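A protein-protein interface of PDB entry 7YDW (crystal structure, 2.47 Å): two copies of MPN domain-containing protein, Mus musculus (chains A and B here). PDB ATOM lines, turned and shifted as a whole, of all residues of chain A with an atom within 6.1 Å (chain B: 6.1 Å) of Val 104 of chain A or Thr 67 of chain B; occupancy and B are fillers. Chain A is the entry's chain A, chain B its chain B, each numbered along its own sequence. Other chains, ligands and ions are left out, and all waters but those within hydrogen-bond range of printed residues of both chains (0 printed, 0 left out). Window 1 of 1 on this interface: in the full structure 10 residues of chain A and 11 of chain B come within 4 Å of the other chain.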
ATOM      1  N   GLU A  81       0.329  -2.569  28.252  1.00  0.00           N
ATOM      2  CA  GLU A  81      -0.925  -2.679  27.471  1.00  0.00           C
ATOM      3  C   GLU A  81      -2.115  -2.797  28.425  1.00  0.00           C
ATOM      4  O   GLU A  81      -1.978  -3.490  29.445  1.00  0.00           O
ATOM      5  CB  GLU A  81      -0.883  -3.899  26.561  1.00  0.00           C
ATOM      6  CG  GLU A  81       0.001  -3.719  25.354  1.00  0.00           C
ATOM      7  CD  GLU A  81      -0.149  -4.872  24.386  1.00  0.00           C
ATOM      8  OE1 GLU A  81       0.403  -5.946  24.676  1.00  0.00           O
ATOM      9  OE2 GLU A  81      -0.871  -4.705  23.382  1.00  0.00           O
ATOM     10  N   THR A  94     -10.189   1.667  27.124  1.00  0.00           N
ATOM     11  CA  THR A  94      -8.930   1.061  27.628  1.00  0.00           C
ATOM     12  C   THR A  94      -7.741   1.649  26.856  1.00  0.00           C
ATOM     13  O   THR A  94      -7.838   1.809  25.627  1.00  0.00           O
ATOM     14  CB  THR A  94      -9.010  -0.471  27.587  1.00  0.00           C
ATOM     15  OG1 THR A  94      -9.139  -0.893  26.231  1.00  0.00           O
ATOM     16  CG2 THR A  94     -10.179  -1.013  28.378  1.00  0.00           C
ATOM     17  N   GLY A  95      -6.667   1.972  27.574  1.00  0.00           N
ATOM     18  CA  GLY A  95      -5.474   2.637  27.028  1.00  0.00           C
ATOM     19  C   GLY A  95      -4.219   1.813  27.255  1.00  0.00           C
ATOM     20  O   GLY A  95      -4.129   1.113  28.293  1.00  0.00           O
ATOM     21  N   ASP A  96      -3.287   1.879  26.307  1.00  0.00           N
ATOM     22  CA  ASP A  96      -1.898   1.380  26.475  1.00  0.00           C
ATOM     23  C   ASP A  96      -1.022   2.573  26.879  1.00  0.00           C
ATOM     24  O   ASP A  96      -1.100   3.624  26.210  1.00  0.00           O
ATOM     25  CB  ASP A  96      -1.384   0.702  25.203  1.00  0.00           C
ATOM     26  CG  ASP A  96      -2.276  -0.405  24.665  1.00  0.00           C
ATOM     27  OD1 ASP A  96      -2.967  -1.056  25.478  1.00  0.00           O
ATOM     28  OD2 ASP A  96      -2.263  -0.611  23.429  1.00  0.00           O
ATOM     29  N   LEU A  97      -0.243   2.433  27.951  1.00  0.00           N
ATOM     30  CA  LEU A  97       0.743   3.460  28.367  1.00  0.00           C
ATOM     31  C   LEU A  97       2.089   3.112  27.728  1.00  0.00           C
ATOM     32  O   LEU A  97       2.599   2.000  27.987  1.00  0.00           O
ATOM     33  CB  LEU A  97       0.833   3.514  29.894  1.00  0.00           C
ATOM     34  CG  LEU A  97       1.763   4.578  30.471  1.00  0.00           C
ATOM     35  CD1 LEU A  97       1.501   5.960  29.879  1.00  0.00           C
ATOM     36  CD2 LEU A  97       1.634   4.623  31.981  1.00  0.00           C
ATOM     37  N   GLN A  98       2.603   4.023  26.894  1.00  0.00           N
ATOM     38  CA  GLN A  98       3.940   3.938  26.245  1.00  0.00           C
ATOM     39  C   GLN A  98       4.981   4.584  27.168  1.00  0.00           C
ATOM     40  O   GLN A  98       4.601   5.459  27.979  1.00  0.00           O
ATOM     41  CB  GLN A  98       3.915   4.611  24.871  1.00  0.00           C
ATOM     42  CG  GLN A  98       2.992   3.920  23.873  1.00  0.00           C
ATOM     43  CD  GLN A  98       3.039   4.539  22.494  1.00  0.00           C
ATOM     44  OE1 GLN A  98       3.406   5.703  22.318  1.00  0.00           O
ATOM     45  NE2 GLN A  98       2.674   3.751  21.493  1.00  0.00           N
ATOM     46  N   ARG A 102       2.863   8.650  26.373  1.00  0.00           N
ATOM     47  CA  ARG A 102       1.709   8.881  25.469  1.00  0.00           C
ATOM     48  C   ARG A 102       0.742   7.694  25.594  1.00  0.00           C
ATOM     49  O   ARG A 102       1.201   6.585  25.931  1.00  0.00           O
ATOM     50  CB  ARG A 102       2.216   9.142  24.048  1.00  0.00           C
ATOM     51  CG  ARG A 102       2.754  10.554  23.870  1.00  0.00           C
ATOM     52  CD  ARG A 102       3.186  10.899  22.463  1.00  0.00           C
ATOM     53  NE  ARG A 102       4.133  12.004  22.498  1.00  0.00           N
ATOM     54  N   ILE A 103      -0.553   7.938  25.362  1.00  0.00           N
ATOM     55  CA  ILE A 103      -1.657   6.951  25.559  1.00  0.00           C
ATOM     56  C   ILE A 103      -2.153   6.484  24.185  1.00  0.00           C
ATOM     57  O   ILE A 103      -2.464   7.348  23.344  1.00  0.00           O
ATOM     58  CB  ILE A 103      -2.791   7.580  26.398  1.00  0.00           C
ATOM     59  CG1 ILE A 103      -2.269   8.134  27.727  1.00  0.00           C
ATOM     60  CG2 ILE A 103      -3.934   6.594  26.610  1.00  0.00           C
ATOM     61  CD1 ILE A 103      -3.268   8.989  28.475  1.00  0.00           C
ATOM     62  N   VAL A 104      -2.228   5.168  23.972  1.00  0.00           N
ATOM     63  CA  VAL A 104      -2.869   4.553  22.775  1.00  0.00           C
ATOM     64  C   VAL A 104      -4.251   4.036  23.182  1.00  0.00           C
ATOM     65  O   VAL A 104      -4.324   3.226  24.116  1.00  0.00           O
ATOM     66  CB  VAL A 104      -2.010   3.423  22.176  1.00  0.00           C
ATOM     67  CG1 VAL A 104      -2.637   2.853  20.910  1.00  0.00           C
ATOM     68  CG2 VAL A 104      -0.591   3.889  21.903  1.00  0.00           C
ATOM     69  N   TRP A 105      -5.305   4.485  22.500  1.00  0.00           N
ATOM     70  CA  TRP A 105      -6.689   4.005  22.730  1.00  0.00           C
ATOM     71  C   TRP A 105      -6.854   2.691  21.962  1.00  0.00           C
ATOM     72  O   TRP A 105      -6.728   2.709  20.727  1.00  0.00           O
ATOM     73  CB  TRP A 105      -7.718   5.085  22.346  1.00  0.00           C
ATOM     74  CG  TRP A 105      -9.146   4.670  22.537  1.00  0.00           C
ATOM     75  CD1 TRP A 105      -9.620   3.693  23.364  1.00  0.00           C
ATOM     76  CD2 TRP A 105     -10.297   5.226  21.883  1.00  0.00           C
ATOM     77  NE1 TRP A 105     -10.978   3.588  23.251  1.00  0.00           N
ATOM     78  CE2 TRP A 105     -11.422   4.523  22.359  1.00  0.00           C
ATOM     79  CE3 TRP A 105     -10.485   6.244  20.942  1.00  0.00           C
ATOM     80  CZ2 TRP A 105     -12.712   4.802  21.918  1.00  0.00           C
ATOM     81  CZ3 TRP A 105     -11.760   6.523  20.510  1.00  0.00           C
ATOM     82  CH2 TRP A 105     -12.856   5.807  20.992  1.00  0.00           C
ATOM     83  N   GLN A 106      -7.084   1.587  22.679  1.00  0.00           N
ATOM     84  CA  GLN A 106      -7.065   0.208  22.116  1.00  0.00           C
ATOM     85  C   GLN A 106      -8.039   0.117  20.934  1.00  0.00           C
ATOM     86  O   GLN A 106      -7.636  -0.419  19.889  1.00  0.00           O
ATOM     87  CB  GLN A 106      -7.356  -0.827  23.206  1.00  0.00           C
ATOM     88  CG  GLN A 106      -6.217  -1.001  24.210  1.00  0.00           C
ATOM     89  CD  GLN A 106      -6.157  -2.370  24.853  1.00  0.00           C
ATOM     90  OE1 GLN A 106      -7.167  -3.030  25.098  1.00  0.00           O
ATOM     91  NE2 GLN A 106      -4.947  -2.817  25.142  1.00  0.00           N
ATOM     92  N   GLU A 107      -9.249   0.671  21.070  1.00  0.00           N
ATOM     93  CA  GLU A 107     -10.353   0.533  20.076  1.00  0.00           C
ATOM     94  C   GLU A 107      -9.918   1.012  18.681  1.00  0.00           C
ATOM     95  O   GLU A 107     -10.264   0.325  17.714  1.00  0.00           O
ATOM     96  CB  GLU A 107     -11.610   1.290  20.510  1.00  0.00           C
ATOM     97  CG  GLU A 107     -12.731   1.211  19.483  1.00  0.00           C
ATOM     98  CD  GLU A 107     -14.125   1.570  19.971  1.00  0.00           C
ATOM     99  OE1 GLU A 107     -14.952   1.972  19.122  1.00  0.00           O
ATOM    100  OE2 GLU A 107     -14.390   1.434  21.186  1.00  0.00           O
ATOM    101  N   THR A 108      -9.224   2.148  18.573  1.00  0.00           N
ATOM    102  CA  THR A 108      -8.890   2.801  17.275  1.00  0.00           C
ATOM    103  C   THR A 108      -7.379   2.891  17.016  1.00  0.00           C
ATOM    104  O   THR A 108      -7.001   3.174  15.857  1.00  0.00           O
ATOM    105  CB  THR A 108      -9.461   4.221  17.218  1.00  0.00           C
ATOM    106  OG1 THR A 108      -8.647   5.049  18.053  1.00  0.00           O
ATOM    107  CG2 THR A 108     -10.921   4.258  17.620  1.00  0.00           C
ATOM    108  N   GLY A 109      -6.551   2.731  18.049  1.00  0.00           N
ATOM    109  CA  GLY A 109      -5.088   2.833  17.931  1.00  0.00           C
ATOM    110  C   GLY A 109      -4.621   4.274  17.892  1.00  0.00           C
ATOM    111  O   GLY A 109      -3.398   4.476  17.818  1.00  0.00           O
ATOM    112  N   GLN A 110      -5.548   5.236  17.955  1.00  0.00           N
ATOM    113  CA  GLN A 110      -5.246   6.693  17.985  1.00  0.00           C
ATOM    114  C   GLN A 110      -4.429   7.008  19.239  1.00  0.00           C
ATOM    115  O   GLN A 110      -4.741   6.444  20.298  1.00  0.00           O
ATOM    116  CB  GLN A 110      -6.528   7.529  17.976  1.00  0.00           C
ATOM    117  CG  GLN A 110      -6.282   9.027  18.132  1.00  0.00           C
ATOM    118  CD  GLN A 110      -7.515   9.849  17.847  1.00  0.00           C
ATOM    119  OE1 GLN A 110      -8.564   9.329  17.458  1.00  0.00           O
ATOM    120  NE2 GLN A 110      -7.398  11.151  18.045  1.00  0.00           N
ATOM    121  N   VAL A 111      -3.434   7.888  19.110  1.00  0.00           N
ATOM    122  CA  VAL A 111      -2.425   8.189  20.165  1.00  0.00           C
ATOM    123  C   VAL A 111      -2.758   9.553  20.762  1.00  0.00           C
ATOM    124  O   VAL A 111      -2.972  10.484  19.978  1.00  0.00           O
ATOM    125  CB  VAL A 111      -0.992   8.160  19.602  1.00  0.00           C
ATOM    126  CG1 VAL A 111       0.048   8.354  20.697  1.00  0.00           C
ATOM    127  CG2 VAL A 111      -0.715   6.873  18.835  1.00  0.00           C
ATOM    128  N   PHE A 112      -2.775   9.650  22.096  1.00  0.00           N
ATOM    129  CA  PHE A 112      -3.037  10.897  22.862  1.00  0.00           C
ATOM    130  C   PHE A 112      -1.815  11.257  23.716  1.00  0.00           C
ATOM    131  O   PHE A 112      -1.121  10.350  24.239  1.00  0.00           O
ATOM    132  CB  PHE A 112      -4.305  10.742  23.700  1.00  0.00           C
ATOM    133  CG  PHE A 112      -5.550  10.537  22.872  1.00  0.00           C
ATOM    134  CD1 PHE A 112      -6.327  11.616  22.481  1.00  0.00           C
ATOM    135  CD2 PHE A 112      -5.929   9.268  22.463  1.00  0.00           C
ATOM    136  CE1 PHE A 112      -7.463  11.430  21.711  1.00  0.00           C
ATOM    137  CE2 PHE A 112      -7.069   9.085  21.696  1.00  0.00           C
ATOM    138  CZ  PHE A 112      -7.834  10.166  21.321  1.00  0.00           C
ATOM    139  N   TRP A 118      -7.235  12.265  26.011  1.00  0.00           N
ATOM    140  CA  TRP A 118      -7.890  10.943  25.821  1.00  0.00           C
ATOM    141  C   TRP A 118      -9.292  10.957  26.445  1.00  0.00           C
ATOM    142  O   TRP A 118     -10.230  10.452  25.793  1.00  0.00           O
ATOM    143  CB  TRP A 118      -7.015   9.820  26.397  1.00  0.00           C
ATOM    144  CG  TRP A 118      -7.585   8.444  26.236  1.00  0.00           C
ATOM    145  CD1 TRP A 118      -8.151   7.907  25.115  1.00  0.00           C
ATOM    146  CD2 TRP A 118      -7.619   7.410  27.234  1.00  0.00           C
ATOM    147  NE1 TRP A 118      -8.550   6.619  25.353  1.00  0.00           N
ATOM    148  CE2 TRP A 118      -8.230   6.285  26.640  1.00  0.00           C
ATOM    149  CE3 TRP A 118      -7.204   7.331  28.567  1.00  0.00           C
ATOM    150  CZ2 TRP A 118      -8.436   5.096  27.338  1.00  0.00           C
ATOM    151  CZ3 TRP A 118      -7.415   6.160  29.257  1.00  0.00           C
ATOM    152  CH2 TRP A 118      -8.026   5.060  28.650  1.00  0.00           C
ATOM    153  N   ALA B  65      -1.161   3.988  16.255  1.00  0.00           N
ATOM    154  CA  ALA B  65      -0.286   2.882  16.707  1.00  0.00           C
ATOM    155  C   ALA B  65      -1.077   1.567  16.695  1.00  0.00           C
ATOM    156  O   ALA B  65      -2.303   1.632  16.871  1.00  0.00           O
ATOM    157  CB  ALA B  65       0.227   3.185  18.094  1.00  0.00           C
ATOM    158  N   VAL B  66      -0.397   0.424  16.529  1.00  0.00           N
ATOM    159  CA  VAL B  66      -1.021  -0.923  16.321  1.00  0.00           C
ATOM    160  C   VAL B  66      -1.639  -1.420  17.631  1.00  0.00           C
ATOM    161  O   VAL B  66      -1.029  -1.201  18.690  1.00  0.00           O
ATOM    162  CB  VAL B  66      -0.003  -1.941  15.769  1.00  0.00           C
ATOM    163  CG1 VAL B  66      -0.561  -3.355  15.737  1.00  0.00           C
ATOM    164  CG2 VAL B  66       0.483  -1.547  14.387  1.00  0.00           C
ATOM    165  N   THR B  67      -2.811  -2.058  17.548  1.00  0.00           N
ATOM    166  CA  THR B  67      -3.439  -2.863  18.633  1.00  0.00           C
ATOM    167  C   THR B  67      -4.112  -4.086  18.001  1.00  0.00           C
ATOM    168  O   THR B  67      -4.364  -4.042  16.780  1.00  0.00           O
ATOM    169  CB  THR B  67      -4.459  -2.051  19.444  1.00  0.00           C
ATOM    170  OG1 THR B  67      -5.583  -1.760  18.613  1.00  0.00           O
ATOM    171  CG2 THR B  67      -3.894  -0.760  19.994  1.00  0.00           C
ATOM    172  N   LEU B  68      -4.426  -5.122  18.787  1.00  0.00           N
ATOM    173  CA  LEU B  68      -5.145  -6.321  18.265  1.00  0.00           C
ATOM    174  C   LEU B  68      -6.423  -5.841  17.562  1.00  0.00           C
ATOM    175  O   LEU B  68      -6.737  -6.383  16.473  1.00  0.00           O
ATOM    176  CB  LEU B  68      -5.441  -7.326  19.393  1.00  0.00           C
ATOM    177  CG  LEU B  68      -4.482  -8.513  19.505  1.00  0.00           C
ATOM    178  N   ARG B  69      -7.086  -4.822  18.130  1.00  0.00           N
ATOM    179  CA  ARG B  69      -8.388  -4.284  17.648  1.00  0.00           C
ATOM    180  C   ARG B  69      -8.202  -3.596  16.290  1.00  0.00           C
ATOM    181  O   ARG B  69      -9.058  -3.814  15.417  1.00  0.00           O
ATOM    182  CB  ARG B  69      -9.011  -3.337  18.680  1.00  0.00           C
ATOM    183  CG  ARG B  69     -10.382  -2.803  18.291  1.00  0.00           C
ATOM    184  CD  ARG B  69     -11.385  -3.883  17.913  1.00  0.00           C
ATOM    185  NE  ARG B  69     -12.698  -3.335  17.593  1.00  0.00           N
ATOM    186  N   VAL B  70      -7.129  -2.816  16.108  1.00  0.00           N
ATOM    187  CA  VAL B  70      -6.776  -2.179  14.797  1.00  0.00           C
ATOM    188  C   VAL B  70      -6.505  -3.287  13.766  1.00  0.00           C
ATOM    189  O   VAL B  70      -6.913  -3.123  12.599  1.00  0.00           O
ATOM    190  CB  VAL B  70      -5.586  -1.204  14.912  1.00  0.00           C
ATOM    191  N   LEU B  71      -5.872  -4.391  14.175  1.00  0.00           N
ATOM    192  CA  LEU B  71      -5.583  -5.541  13.273  1.00  0.00           C
ATOM    193  C   LEU B  71      -6.906  -6.190  12.859  1.00  0.00           C
ATOM    194  O   LEU B  71      -7.003  -6.631  11.700  1.00  0.00           O
ATOM    195  CB  LEU B  71      -4.669  -6.563  13.963  1.00  0.00           C
ATOM    196  CG  LEU B  71      -3.247  -6.106  14.281  1.00  0.00           C
ATOM    197  CD1 LEU B  71      -2.479  -7.229  14.949  1.00  0.00           C
ATOM    198  CD2 LEU B  71      -2.504  -5.628  13.037  1.00  0.00           C
ATOM    199  N   LEU B  72      -7.876  -6.251  13.778  1.00  0.00           N
ATOM    200  CA  LEU B  72      -9.206  -6.855  13.514  1.00  0.00           C
ATOM    201  C   LEU B  72      -9.984  -5.982  12.519  1.00  0.00           C
ATOM    202  O   LEU B  72     -10.544  -6.566  11.571  1.00  0.00           O
ATOM    203  CB  LEU B  72      -9.955  -7.053  14.834  1.00  0.00           C
ATOM    204  CG  LEU B  72      -9.546  -8.299  15.621  1.00  0.00           C
ATOM    205  CD1 LEU B  72      -9.991  -8.210  17.078  1.00  0.00           C
ATOM    206  CD2 LEU B  72     -10.092  -9.561  14.964  1.00  0.00           C
ATOM    207  N   TRP B 136       4.090  -9.462  22.575  1.00  0.00           N
ATOM    208  CA  TRP B 136       3.811  -9.614  21.122  1.00  0.00           C
ATOM    209  C   TRP B 136       4.859 -10.547  20.494  1.00  0.00           C
ATOM    210  O   TRP B 136       4.475 -11.351  19.612  1.00  0.00           O
ATOM    211  CB  TRP B 136       3.718  -8.260  20.407  1.00  0.00           C
ATOM    212  CG  TRP B 136       2.394  -7.581  20.580  1.00  0.00           C
ATOM    213  CD1 TRP B 136       1.824  -7.192  21.760  1.00  0.00           C
ATOM    214  CD2 TRP B 136       1.463  -7.206  19.546  1.00  0.00           C
ATOM    215  NE1 TRP B 136       0.613  -6.602  21.528  1.00  0.00           N
ATOM    216  CE2 TRP B 136       0.363  -6.594  20.183  1.00  0.00           C
ATOM    217  CE3 TRP B 136       1.448  -7.324  18.152  1.00  0.00           C
ATOM    218  CZ2 TRP B 136      -0.732  -6.104  19.477  1.00  0.00           C
ATOM    219  CZ3 TRP B 136       0.369  -6.832  17.450  1.00  0.00           C
ATOM    220  CH2 TRP B 136      -0.708  -6.230  18.107  1.00  0.00           C
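O of Gly 109 of chain A is in hydrogen-bond range of N of Ala 65 of chain B.
OG1 of Thr 67 of chain B sits at hydrogen-bond distance from O of Gln 106 of chain A (2.8 Å).
OE2 of Glu 81 of chain A sits at hydrogen-bond distance from NE1 of Trp 136 of chain B (3.0 Å).
The side-chain carboxylate (OD1) of Asp 96 of chain A is in hydrogen-bond range of the side-chain amide nitrogen (NE2) of Gln 106 of chain A.
The side-chain hydroxyl (OG1) of Thr 67 of chain B sits close to the backbone NH (N) of Arg 69 of chain B (3.4 Å).
The backbone carbonyl oxygen of Thr 94 of chain A sits at hydrogen-bond distance from the backbone NH of Gln 106 of chain A (3.1 Å).
The side-chain hydroxyl (OG1) of Thr 67 of chain B is in hydrogen-bond range of the backbone NH (N) of Val 70 of chain B (3.1 Å).
The backbone NH (N) of Asp 96 of chain A is in hydrogen-bond range of the backbone carbonyl oxygen (O) of Val 104 of chain A, 2.8 Å away.
Among the printed residues, pairs that only touch across the chains: Glu 107 of chain A with Arg 69 of chain B, Gln 106 of chain A with Arg 69 of chain B, Asp 96 of chain A with Thr 67 of chain B, Val 111 of chain A with Ala 65 of chain B, Val 104 of chain A with Thr 67 of chain B and Val 104 of chain A with Ala 65 of chain B.
Val 104 of chain A touches just these residues of chain B: Ala 65 and Thr 67.
Printed residues of chain A within 4 Å of Ala 65 of chain B: Val 104 (3.96 Å), Gly 109 (2.8 Å) and Val 111 (3.9 Å).
Of the printed residues of chain B, Asp 96 of chain A touches Thr 67.
Of the printed residues of chain B, Glu 107 of chain A touches Arg 69.
Arg 102 of chain A touches none of the printed residues of chain B.
The nearest residue of chain B that does not touch Val 104 of chain A is Val 66 of chain B (4.9 Å).
The nearest printed residue of chain B that does not touch Glu 107 of chain A is Val 70 of chain B (4.7 Å).
Printed residues of chain A that touch a printed residue of chain B: Glu 81, Asp 96, Val 104, Gln 106, Glu 107, Gly 109 and Val 111.
Hydrophobic or aromatic side chains of chain A that line the printed part of chain B: Val 104 and Val 111.
Among the printed residues, no Asp or Glu carboxylate lies within 4 Å of a Lys or Arg side-chain nitrogen of the other chain.
No position is printed for both chains.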
